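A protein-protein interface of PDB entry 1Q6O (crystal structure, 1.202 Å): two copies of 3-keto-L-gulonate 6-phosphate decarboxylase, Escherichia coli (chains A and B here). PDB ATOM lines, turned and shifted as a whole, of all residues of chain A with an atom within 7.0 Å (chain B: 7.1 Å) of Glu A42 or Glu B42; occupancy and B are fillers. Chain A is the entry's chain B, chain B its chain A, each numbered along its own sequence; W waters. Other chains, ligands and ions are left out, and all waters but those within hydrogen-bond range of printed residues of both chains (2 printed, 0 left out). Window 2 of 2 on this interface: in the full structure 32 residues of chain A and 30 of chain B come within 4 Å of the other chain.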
ATOM      1  N   ASN A  12      36.092   1.617 -22.003  1.00  0.00           N
ATOM      2  CA  ASN A  12      35.307   1.145 -23.150  1.00  0.00           C
ATOM      3  C   ASN A  12      33.975   0.685 -22.635  1.00  0.00           C
ATOM      4  O   ASN A  12      33.832   0.353 -21.473  1.00  0.00           O
ATOM      5  CB  ASN A  12      36.026  -0.068 -23.792  1.00  0.00           C
ATOM      6  CG  ASN A  12      37.428   0.277 -24.324  1.00  0.00           C
ATOM      7  OD1 ASN A  12      37.590   0.653 -25.493  1.00  0.00           O
ATOM      8  ND2 ASN A  12      38.442   0.149 -23.483  1.00  0.00           N
ATOM      9  N   GLN A  13      32.961   0.730 -23.513  1.00  0.00           N
ATOM     10  CA  GLN A  13      31.617   0.356 -23.130  1.00  0.00           C
ATOM     11  C   GLN A  13      31.299  -1.123 -23.312  1.00  0.00           C
ATOM     12  O   GLN A  13      30.384  -1.630 -22.692  1.00  0.00           O
ATOM     13  CB  GLN A  13      30.595   1.228 -23.879  1.00  0.00           C
ATOM     14  CG  GLN A  13      30.831   2.696 -23.589  1.00  0.00           C
ATOM     15  CD  GLN A  13      29.789   3.650 -24.105  1.00  0.00           C
ATOM     16  OE1 GLN A  13      30.085   4.857 -24.234  1.00  0.00           O
ATOM     17  NE2 GLN A  13      28.588   3.159 -24.352  1.00  0.00           N
ATOM     18  N   THR A  14      32.091  -1.826 -24.135  1.00  0.00           N
ATOM     19  CA  THR A  14      31.925  -3.250 -24.388  1.00  0.00           C
ATOM     20  C   THR A  14      33.268  -3.937 -24.441  1.00  0.00           C
ATOM     21  O   THR A  14      34.319  -3.321 -24.724  1.00  0.00           O
ATOM     22  CB  THR A  14      31.222  -3.533 -25.731  1.00  0.00           C
ATOM     23  OG1 THR A  14      31.997  -2.965 -26.801  1.00  0.00           O
ATOM     24  CG2 THR A  14      29.804  -2.891 -25.777  1.00  0.00           C
ATOM     25  N   MET A  15      33.242  -5.242 -24.206  1.00  0.00           N
ATOM     26  CA  MET A  15      34.480  -6.004 -24.177  1.00  0.00           C
ATOM     27  C   MET A  15      35.163  -5.988 -25.527  1.00  0.00           C
ATOM     28  O   MET A  15      36.380  -5.922 -25.578  1.00  0.00           O
ATOM     29  CB  MET A  15      34.270  -7.490 -23.762  1.00  0.00           C
ATOM     30  CG  MET A  15      33.670  -7.755 -22.411  1.00  0.00           C
ATOM     31  SD  MET A  15      34.492  -6.864 -21.119  1.00  0.00           S
ATOM     32  CE  MET A  15      36.230  -7.377 -21.200  1.00  0.00           C
ATOM     33  N   ASP A  16      34.415  -6.081 -26.627  1.00  0.00           N
ATOM     34  CA  ASP A  16      35.077  -6.163 -27.936  1.00  0.00           C
ATOM     35  C   ASP A  16      35.872  -4.899 -28.249  1.00  0.00           C
ATOM     36  O   ASP A  16      36.959  -4.959 -28.822  1.00  0.00           O
ATOM     37  CB  ASP A  16      34.078  -6.520 -29.040  1.00  0.00           C
ATOM     38  CG  ASP A  16      33.041  -5.470 -29.247  1.00  0.00           C
ATOM     39  OD1 ASP A  16      32.248  -5.262 -28.316  1.00  0.00           O
ATOM     40  OD2 ASP A  16      32.981  -4.825 -30.303  1.00  0.00           O
ATOM     41  N   SER A  17      35.346  -3.749 -27.818  1.00  0.00           N
ATOM     42  CA  SER A  17      36.056  -2.490 -27.963  1.00  0.00           C
ATOM     43  C   SER A  17      37.342  -2.521 -27.109  1.00  0.00           C
ATOM     44  O   SER A  17      38.406  -2.132 -27.572  1.00  0.00           O
ATOM     45  CB  SER A  17      35.137  -1.350 -27.553  1.00  0.00           C
ATOM     46  OG  SER A  17      35.786  -0.106 -27.576  1.00  0.00           O
ATOM     47  N   THR A  36      36.003   2.269 -15.194  1.00  0.00           N
ATOM     48  CA  THR A  36      34.689   2.370 -14.586  1.00  0.00           C
ATOM     49  C   THR A  36      33.598   2.220 -15.633  1.00  0.00           C
ATOM     50  O   THR A  36      32.592   1.551 -15.407  1.00  0.00           O
ATOM     51  CB  THR A  36      34.528   3.704 -13.859  1.00  0.00           C
ATOM     52  OG1 THR A  36      35.677   3.959 -13.053  1.00  0.00           O
ATOM     53  CG2 THR A  36      33.323   3.700 -12.919  1.00  0.00           C
ATOM     54  N   ILE A  37      33.755   2.825 -16.795  1.00  0.00           N
ATOM     55  CA  ILE A  37      32.641   2.685 -17.753  1.00  0.00           C
ATOM     56  C   ILE A  37      32.559   1.275 -18.309  1.00  0.00           C
ATOM     57  O   ILE A  37      31.485   0.884 -18.742  1.00  0.00           O
ATOM     58  CB  ILE A  37      32.678   3.517 -18.961  1.00  0.00           C
ATOM     59  CG1 ILE A  37      31.345   3.645 -19.723  1.00  0.00           C
ATOM     60  CG2 ILE A  37      33.962   3.519 -19.566  1.00  0.00           C
ATOM     61  CD1 ILE A  37      31.253   4.939 -20.539  1.00  0.00           C
ATOM     62  N   LEU A  38      33.674   0.541 -18.366  1.00  0.00           N
ATOM     63  CA  LEU A  38      33.587  -0.879 -18.756  1.00  0.00           C
ATOM     64  C   LEU A  38      32.941  -1.695 -17.616  1.00  0.00           C
ATOM     65  O   LEU A  38      32.148  -2.619 -17.877  1.00  0.00           O
ATOM     66  CB  LEU A  38      34.967  -1.408 -19.154  1.00  0.00           C
ATOM     67  CG  LEU A  38      35.037  -2.802 -19.766  1.00  0.00           C
ATOM     68  CD1 LEU A  38      34.159  -2.941 -21.004  1.00  0.00           C
ATOM     69  CD2 LEU A  38      36.468  -3.175 -20.097  1.00  0.00           C
ATOM     70  N   CYS A  39      33.244  -1.383 -16.371  1.00  0.00           N
ATOM     71  CA  CYS A  39      32.589  -2.047 -15.230  1.00  0.00           C
ATOM     72  C   CYS A  39      31.068  -1.826 -15.303  1.00  0.00           C
ATOM     73  O   CYS A  39      30.291  -2.751 -15.071  1.00  0.00           O
ATOM     74  CB  CYS A  39      33.095  -1.497 -13.904  1.00  0.00           C
ATOM     75  SG  CYS A  39      34.765  -1.900 -13.354  1.00  0.00           S
ATOM     76  N   VAL A  40      30.636  -0.609 -15.621  1.00  0.00           N
ATOM     77  CA  VAL A  40      29.213  -0.280 -15.683  1.00  0.00           C
ATOM     78  C   VAL A  40      28.610  -0.784 -16.994  1.00  0.00           C
ATOM     79  O   VAL A  40      27.429  -1.136 -17.025  1.00  0.00           O
ATOM     80  CB  VAL A  40      28.954   1.265 -15.511  1.00  0.00           C
ATOM     81  CG1 VAL A  40      27.455   1.551 -15.628  1.00  0.00           C
ATOM     82  CG2 VAL A  40      29.430   1.751 -14.176  1.00  0.00           C
ATOM     83  N   GLY A  41      29.389  -0.820 -18.062  1.00  0.00           N
ATOM     84  CA  GLY A  41      28.943  -1.266 -19.365  1.00  0.00           C
ATOM     85  C   GLY A  41      28.691  -2.781 -19.468  1.00  0.00           C
ATOM     86  O   GLY A  41      27.663  -3.227 -19.980  1.00  0.00           O
ATOM     87  N   GLU A  42      29.634  -3.560 -18.955  1.00  0.00           N
ATOM     88  CA  GLU A  42      29.602  -5.023 -19.052  1.00  0.00           C
ATOM     89  C   GLU A  42      29.426  -5.728 -17.719  1.00  0.00           C
ATOM     90  O   GLU A  42      29.087  -6.923 -17.682  1.00  0.00           O
ATOM     91  CB  GLU A  42      30.891  -5.496 -19.693  1.00  0.00           C
ATOM     92  CG  GLU A  42      31.016  -5.135 -21.140  1.00  0.00           C
ATOM     93  CD  GLU A  42      30.270  -6.053 -22.096  1.00  0.00           C
ATOM     94  OE1 GLU A  42      29.323  -6.755 -21.695  1.00  0.00           O
ATOM     95  OE2 GLU A  42      30.652  -6.103 -23.262  1.00  0.00           O
ATOM     96  N   GLY A  43      29.669  -5.048 -16.628  1.00  0.00           N
ATOM     97  CA  GLY A  43      29.660  -5.674 -15.336  1.00  0.00           C
ATOM     98  C   GLY A  43      30.932  -6.462 -15.114  1.00  0.00           C
ATOM     99  O   GLY A  43      31.899  -6.409 -15.910  1.00  0.00           O
ATOM    100  N   VAL A  44      30.954  -7.181 -14.019  1.00  0.00           N
ATOM    101  CA  VAL A  44      32.164  -7.775 -13.521  1.00  0.00           C
ATOM    102  C   VAL A  44      32.706  -8.912 -14.401  1.00  0.00           C
ATOM    103  O   VAL A  44      33.854  -9.328 -14.239  1.00  0.00           O
ATOM    104  CB  VAL A  44      31.946  -8.157 -12.060  1.00  0.00           C
ATOM    105  CG1 VAL A  44      31.067  -9.382 -11.903  1.00  0.00           C
ATOM    106  CG2 VAL A  44      33.228  -8.282 -11.351  1.00  0.00           C
ATOM    107  N   ARG A  45      31.907  -9.393 -15.338  1.00  0.00           N
ATOM    108  CA  ARG A  45      32.462 -10.301 -16.326  1.00  0.00           C
ATOM    109  C   ARG A  45      33.684  -9.701 -17.025  1.00  0.00           C
ATOM    110  O   ARG A  45      34.538 -10.436 -17.506  1.00  0.00           O
ATOM    111  CB  ARG A  45      31.403 -10.721 -17.336  1.00  0.00           C
ATOM    112  CG  ARG A  45      31.056  -9.674 -18.324  1.00  0.00           C
ATOM    113  CD  ARG A  45      30.361 -10.165 -19.610  1.00  0.00           C
ATOM    114  NE  ARG A  45      31.139 -11.228 -20.250  1.00  0.00           N
ATOM    115  CZ  ARG A  45      30.682 -12.451 -20.582  1.00  0.00           C
ATOM    116  NH1 ARG A  45      29.414 -12.843 -20.411  1.00  0.00           N
ATOM    117  NH2 ARG A  45      31.530 -13.304 -21.117  1.00  0.00           N
ATOM    118  N   ALA A  46      33.777  -8.376 -17.115  1.00  0.00           N
ATOM    119  CA  ALA A  46      34.912  -7.752 -17.753  1.00  0.00           C
ATOM    120  C   ALA A  46      36.197  -8.102 -17.040  1.00  0.00           C
ATOM    121  O   ALA A  46      37.222  -8.334 -17.679  1.00  0.00           O
ATOM    122  CB  ALA A  46      34.728  -6.242 -17.800  1.00  0.00           C
ATOM    123  N   MET A  75      32.688  -9.094  -5.110  1.00  0.00           N
ATOM    124  CA  MET A  75      32.289  -9.346  -6.496  1.00  0.00           C
ATOM    125  C   MET A  75      33.492  -9.214  -7.424  1.00  0.00           C
ATOM    126  O   MET A  75      33.687 -10.035  -8.309  1.00  0.00           O
ATOM    127  CB  MET A  75      31.190  -8.393  -6.905  1.00  0.00           C
ATOM    128  CG  MET A  75      29.894  -8.640  -6.218  1.00  0.00           C
ATOM    129  SD  MET A  75      28.674  -7.330  -6.447  1.00  0.00           S
ATOM    130  CE  MET A  75      28.446  -7.717  -8.292  1.00  0.00           C
ATOM    131  N   ASN B  12      21.185  -6.390  -6.201  1.00  0.00           N
ATOM    132  CA  ASN B  12      21.302  -7.817  -6.498  1.00  0.00           C
ATOM    133  C   ASN B  12      22.487  -7.929  -7.418  1.00  0.00           C
ATOM    134  O   ASN B  12      22.794  -7.023  -8.159  1.00  0.00           O
ATOM    135  CB  ASN B  12      20.026  -8.295  -7.224  1.00  0.00           C
ATOM    136  CG  ASN B  12      18.768  -8.102  -6.413  1.00  0.00           C
ATOM    137  OD1 ASN B  12      18.170  -7.031  -6.396  1.00  0.00           O
ATOM    138  ND2 ASN B  12      18.350  -9.156  -5.745  1.00  0.00           N
ATOM    139  N   GLN B  13      23.124  -9.099  -7.425  1.00  0.00           N
ATOM    140  CA  GLN B  13      24.284  -9.332  -8.271  1.00  0.00           C
ATOM    141  C   GLN B  13      23.961  -9.811  -9.679  1.00  0.00           C
ATOM    142  O   GLN B  13      24.794  -9.648 -10.576  1.00  0.00           O
ATOM    143  CB  GLN B  13      25.263 -10.304  -7.606  1.00  0.00           C
ATOM    144  CG  GLN B  13      25.678  -9.797  -6.245  1.00  0.00           C
ATOM    145  CD  GLN B  13      26.823 -10.511  -5.612  1.00  0.00           C
ATOM    146  OE1 GLN B  13      26.994 -10.404  -4.388  1.00  0.00           O
ATOM    147  NE2 GLN B  13      27.632 -11.197  -6.410  1.00  0.00           N
ATOM    148  N   THR B  14      22.763 -10.380  -9.870  1.00  0.00           N
ATOM    149  CA  THR B  14      22.331 -10.862 -11.175  1.00  0.00           C
ATOM    150  C   THR B  14      20.892 -10.482 -11.439  1.00  0.00           C
ATOM    151  O   THR B  14      20.103 -10.226 -10.512  1.00  0.00           O
ATOM    152  CB  THR B  14      22.426 -12.385 -11.289  1.00  0.00           C
ATOM    153  OG1 THR B  14      21.600 -12.983 -10.288  1.00  0.00           O
ATOM    154  CG2 THR B  14      23.856 -12.889 -11.070  1.00  0.00           C
ATOM    155  N   MET B  15      20.524 -10.480 -12.717  1.00  0.00           N
ATOM    156  CA  MET B  15      19.172 -10.108 -13.089  1.00  0.00           C
ATOM    157  C   MET B  15      18.170 -11.077 -12.508  1.00  0.00           C
ATOM    158  O   MET B  15      17.114 -10.649 -12.050  1.00  0.00           O
ATOM    159  CB  MET B  15      18.942 -10.005 -14.612  1.00  0.00           C
ATOM    160  CG  MET B  15      19.746  -9.009 -15.411  1.00  0.00           C
ATOM    161  SD  MET B  15      19.736  -7.373 -14.673  1.00  0.00           S
ATOM    162  CE  MET B  15      18.003  -6.887 -14.670  1.00  0.00           C
ATOM    163  N   ASP B  16      18.439 -12.373 -12.567  1.00  0.00           N
ATOM    164  CA  ASP B  16      17.456 -13.335 -12.088  1.00  0.00           C
ATOM    165  C   ASP B  16      17.169 -13.167 -10.602  1.00  0.00           C
ATOM    166  O   ASP B  16      16.025 -13.328 -10.173  1.00  0.00           O
ATOM    167  CB  ASP B  16      17.819 -14.782 -12.444  1.00  0.00           C
ATOM    168  CG  ASP B  16      19.099 -15.246 -11.816  1.00  0.00           C
ATOM    169  OD1 ASP B  16      20.142 -14.588 -11.994  1.00  0.00           O
ATOM    170  OD2 ASP B  16      19.136 -16.299 -11.166  1.00  0.00           O
ATOM    171  N   SER B  17      18.193 -12.823  -9.814  1.00  0.00           N
ATOM    172  CA  SER B  17      17.998 -12.487  -8.412  1.00  0.00           C
ATOM    173  C   SER B  17      17.079 -11.233  -8.265  1.00  0.00           C
ATOM    174  O   SER B  17      16.161 -11.216  -7.439  1.00  0.00           O
ATOM    175  CB  SER B  17      19.361 -12.272  -7.737  1.00  0.00           C
ATOM    176  OG  SER B  17      19.226 -11.835  -6.408  1.00  0.00           O
ATOM    177  N   THR B  36      23.637  -0.004  -7.405  1.00  0.00           N
ATOM    178  CA  THR B  36      25.018  -0.006  -7.820  1.00  0.00           C
ATOM    179  C   THR B  36      25.557  -1.430  -7.942  1.00  0.00           C
ATOM    180  O   THR B  36      26.310  -1.738  -8.864  1.00  0.00           O
ATOM    181  CB  THR B  36      25.864   0.819  -6.836  1.00  0.00           C
ATOM    182  OG1 THR B  36      25.220   2.084  -6.566  1.00  0.00           O
ATOM    183  CG2 THR B  36      27.252   1.101  -7.429  1.00  0.00           C
ATOM    184  N   ILE B  37      25.153  -2.301  -7.026  1.00  0.00           N
ATOM    185  CA  ILE B  37      25.571  -3.687  -7.010  1.00  0.00           C
ATOM    186  C   ILE B  37      25.124  -4.404  -8.292  1.00  0.00           C
ATOM    187  O   ILE B  37      25.869  -5.201  -8.848  1.00  0.00           O
ATOM    188  CB  ILE B  37      25.040  -4.363  -5.672  1.00  0.00           C
ATOM    189  CG1 ILE B  37      25.851  -3.764  -4.472  1.00  0.00           C
ATOM    190  CG2 ILE B  37      25.150  -5.868  -5.707  1.00  0.00           C
ATOM    191  CD1 ILE B  37      25.196  -3.822  -3.055  1.00  0.00           C
ATOM    192  N   LEU B  38      23.916  -4.117  -8.764  1.00  0.00           N
ATOM    193  CA  LEU B  38      23.413  -4.709  -9.991  1.00  0.00           C
ATOM    194  C   LEU B  38      24.080  -4.093 -11.225  1.00  0.00           C
ATOM    195  O   LEU B  38      24.370  -4.829 -12.161  1.00  0.00           O
ATOM    196  CB  LEU B  38      21.889  -4.604 -10.029  1.00  0.00           C
ATOM    197  CG  LEU B  38      21.207  -5.324 -11.170  1.00  0.00           C
ATOM    198  CD1 LEU B  38      21.528  -6.808 -11.183  1.00  0.00           C
ATOM    199  CD2 LEU B  38      19.695  -5.117 -11.060  1.00  0.00           C
ATOM    200  N   CYS B  39      24.389  -2.806 -11.221  1.00  0.00           N
ATOM    201  CA  CYS B  39      25.115  -2.165 -12.303  1.00  0.00           C
ATOM    202  C   CYS B  39      26.484  -2.851 -12.409  1.00  0.00           C
ATOM    203  O   CYS B  39      26.945  -3.135 -13.501  1.00  0.00           O
ATOM    204  CB  CYS B  39      25.312  -0.665 -12.022  1.00  0.00           C
ATOM    205  SG  CYS B  39      23.858   0.444 -12.102  1.00  0.00           S
ATOM    206  N   VAL B  40      27.157  -3.097 -11.288  1.00  0.00           N
ATOM    207  CA  VAL B  40      28.457  -3.744 -11.319  1.00  0.00           C
ATOM    208  C   VAL B  40      28.347  -5.231 -11.654  1.00  0.00           C
ATOM    209  O   VAL B  40      29.240  -5.774 -12.304  1.00  0.00           O
ATOM    210  CB  VAL B  40      29.229  -3.464  -9.988  1.00  0.00           C
ATOM    211  CG1 VAL B  40      30.512  -4.286  -9.881  1.00  0.00           C
ATOM    212  CG2 VAL B  40      29.540  -1.978  -9.906  1.00  0.00           C
ATOM    213  N   GLY B  41      27.300  -5.903 -11.219  1.00  0.00           N
ATOM    214  CA  GLY B  41      27.134  -7.305 -11.497  1.00  0.00           C
ATOM    215  C   GLY B  41      26.850  -7.600 -12.954  1.00  0.00           C
ATOM    216  O   GLY B  41      27.440  -8.519 -13.529  1.00  0.00           O
ATOM    217  N   GLU B  42      25.913  -6.854 -13.546  1.00  0.00           N
ATOM    218  CA  GLU B  42      25.368  -7.150 -14.877  1.00  0.00           C
ATOM    219  C   GLU B  42      25.658  -6.084 -15.927  1.00  0.00           C
ATOM    220  O   GLU B  42      25.516  -6.324 -17.141  1.00  0.00           O
ATOM    221  CB  GLU B  42      23.851  -7.344 -14.782  1.00  0.00           C
ATOM    222  CG  GLU B  42      23.410  -8.568 -14.010  1.00  0.00           C
ATOM    223  CD  GLU B  42      23.449  -9.851 -14.821  1.00  0.00           C
ATOM    224  OE1 GLU B  42      24.211  -9.931 -15.816  1.00  0.00           O
ATOM    225  OE2 GLU B  42      22.752 -10.806 -14.469  1.00  0.00           O
ATOM    226  N   GLY B  43      26.037  -4.904 -15.494  1.00  0.00           N
ATOM    227  CA  GLY B  43      26.180  -3.773 -16.381  1.00  0.00           C
ATOM    228  C   GLY B  43      24.853  -3.162 -16.786  1.00  0.00           C
ATOM    229  O   GLY B  43      23.793  -3.529 -16.272  1.00  0.00           O
ATOM    230  N   VAL B  44      24.929  -2.233 -17.708  1.00  0.00           N
ATOM    231  CA  VAL B  44      23.832  -1.373 -18.035  1.00  0.00           C
ATOM    232  C   VAL B  44      22.682  -2.104 -18.746  1.00  0.00           C
ATOM    233  O   VAL B  44      21.575  -1.590 -18.818  1.00  0.00           O
ATOM    234  CB  VAL B  44      24.385  -0.182 -18.839  1.00  0.00           C
ATOM    235  CG1 VAL B  44      24.749  -0.573 -20.262  1.00  0.00           C
ATOM    236  CG2 VAL B  44      23.476   0.974 -18.771  1.00  0.00           C
ATOM    237  N   ARG B  45      22.911  -3.327 -19.196  1.00  0.00           N
ATOM    238  CA  ARG B  45      21.795  -4.120 -19.660  1.00  0.00           C
ATOM    239  C   ARG B  45      20.712  -4.235 -18.569  1.00  0.00           C
ATOM    240  O   ARG B  45      19.548  -4.443 -18.899  1.00  0.00           O
ATOM    241  CB  ARG B  45      22.248  -5.508 -20.097  1.00  0.00           C
ATOM    242  CG  ARG B  45      22.709  -6.391 -18.961  1.00  0.00           C
ATOM    243  CD  ARG B  45      22.677  -7.916 -19.208  1.00  0.00           C
ATOM    244  NE  ARG B  45      21.420  -8.323 -19.825  1.00  0.00           N
ATOM    245  CZ  ARG B  45      21.301  -8.920 -21.011  1.00  0.00           C
ATOM    246  NH1 ARG B  45      22.339  -9.296 -21.777  1.00  0.00           N
ATOM    247  NH2 ARG B  45      20.082  -9.168 -21.423  1.00  0.00           N
ATOM    248  N   ALA B  46      21.079  -4.127 -17.292  1.00  0.00           N
ATOM    249  CA  ALA B  46      20.110  -4.234 -16.238  1.00  0.00           C
ATOM    250  C   ALA B  46      19.072  -3.113 -16.337  1.00  0.00           C
ATOM    251  O   ALA B  46      17.885  -3.313 -16.085  1.00  0.00           O
ATOM    252  CB  ALA B  46      20.815  -4.180 -14.903  1.00  0.00           C
ATOM    253  N   MET B  75      25.447   6.564 -21.575  1.00  0.00           N
ATOM    254  CA  MET B  75      25.297   5.098 -21.566  1.00  0.00           C
ATOM    255  C   MET B  75      24.028   4.674 -20.810  1.00  0.00           C
ATOM    256  O   MET B  75      23.263   3.846 -21.268  1.00  0.00           O
ATOM    257  CB  MET B  75      26.491   4.443 -20.908  1.00  0.00           C
ATOM    258  CG  MET B  75      26.753   3.000 -21.419  1.00  0.00           C
ATOM    259  SD  MET B  75      28.175   2.106 -20.779  1.00  0.00           S
ATOM    260  CE  MET B  75      27.925   2.209 -19.096  1.00  0.00           C
HETATM  261  O   HOH W   1      25.481  -4.879 -19.604  1.00  0.00           O
HETATM  262  O   HOH W   2      28.945  -9.055 -15.809  1.00  0.00           O
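Water W1 lies within hydrogen-bond range of the backbone carbonyl oxygen of Gly A41 (2.8 Å), the backbone carbonyl oxygen of Glu B42 (2.9 Å), the backbone NH of Arg B45 (3.0 Å) and the backbone NH of Val B44 (3.3 Å).
Water W2 lies within hydrogen-bond range of O of Gly B41, O of Glu A42, N of Arg A45 and N of Val A44.
Gln A13 touches Met B75, and with the chains exchanged Met A75 touches Gln B13.
Cys B39 touches its own counterpart, Cys A39.
Gly A41 touches Val B44, and with the chains exchanged Val A44 touches Gly B41.
Glu B42 touches its own counterpart, Glu A42.
Positions printed for both chains: 12, 13, 14, 15, 16, 17, 36, 37, 38, 39, 40, 41, 42, 43, 44, 45, 46 and 75.
Of the 17 pairs that touch across the chains among the printed residues, 15 have their exchanged pair printed and touching as well.
SD of Met B75 lies close to NE2 of Gln A13 (3.7 Å).
The backbone NH (N) of Val B44 lies within hydrogen-bond range of the backbone carbonyl oxygen (O) of Val A40.
O of Val B40 lies within hydrogen-bond range of N of Val A44.
N of Met B15 is in hydrogen-bond range of OE2 of Glu B42.
The backbone NH (N) of Met A15 sits at hydrogen-bond distance from the side-chain carboxylate (OE2) of Glu A42.
Among the printed residues, merely in contact across the chains: Ile A37 with Met B75, Cys A39 with Cys B39, Val A40 with Gly B43, Val A40 with Met B75, Gly A41 with Gly B43, Gly A41 with Val B44, Gly A41 with Met B75, Glu A42 with Glu B42, Gly A43 with Val B40, Gly A43 with Gly B43, Val A44 with Gly B41, Met A75 with Gln B13, Met A75 with Ile B37 and Met A75 with Gly B41.
Asn A12 touches none of the printed residues of chain B.
Printed residues of chain B within 4 Å of Ile A37: Met B75.
Printed residues of chain B within 4 Å of Gly A41: Gly B43, Val B44 and Met B75.
Of the printed residues of chain B, Glu A42 touches Glu B42 (3.7 Å).
Of the printed residues of chain A, Glu B42 touches Glu A42.
Arg B45 touches none of the printed residues of chain A.
Of the 18 printed residues of chain A, 9 touch a printed residue of chain B.
Hydrophobic or aromatic side chains of chain A that line the printed part of chain B: Ile A37, Val A40, Val A44 and Met A75.
Printed residues of chain B that touch a printed residue of chain A: Gln B13, Ile B37, Cys B39, Val B40, Gly B41, Glu B42, Gly B43, Val B44 and Met B75.
Hydrophobic or aromatic side chains of chain B that line the printed part of chain A: Ile B37, Val B44 and Met B75.
Among the printed residues, 17 pairs touch across the chains.
Among the printed residues, no Asp or Glu carboxylate lies within 4 Å of a Lys or Arg side-chain nitrogen of the other chain.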
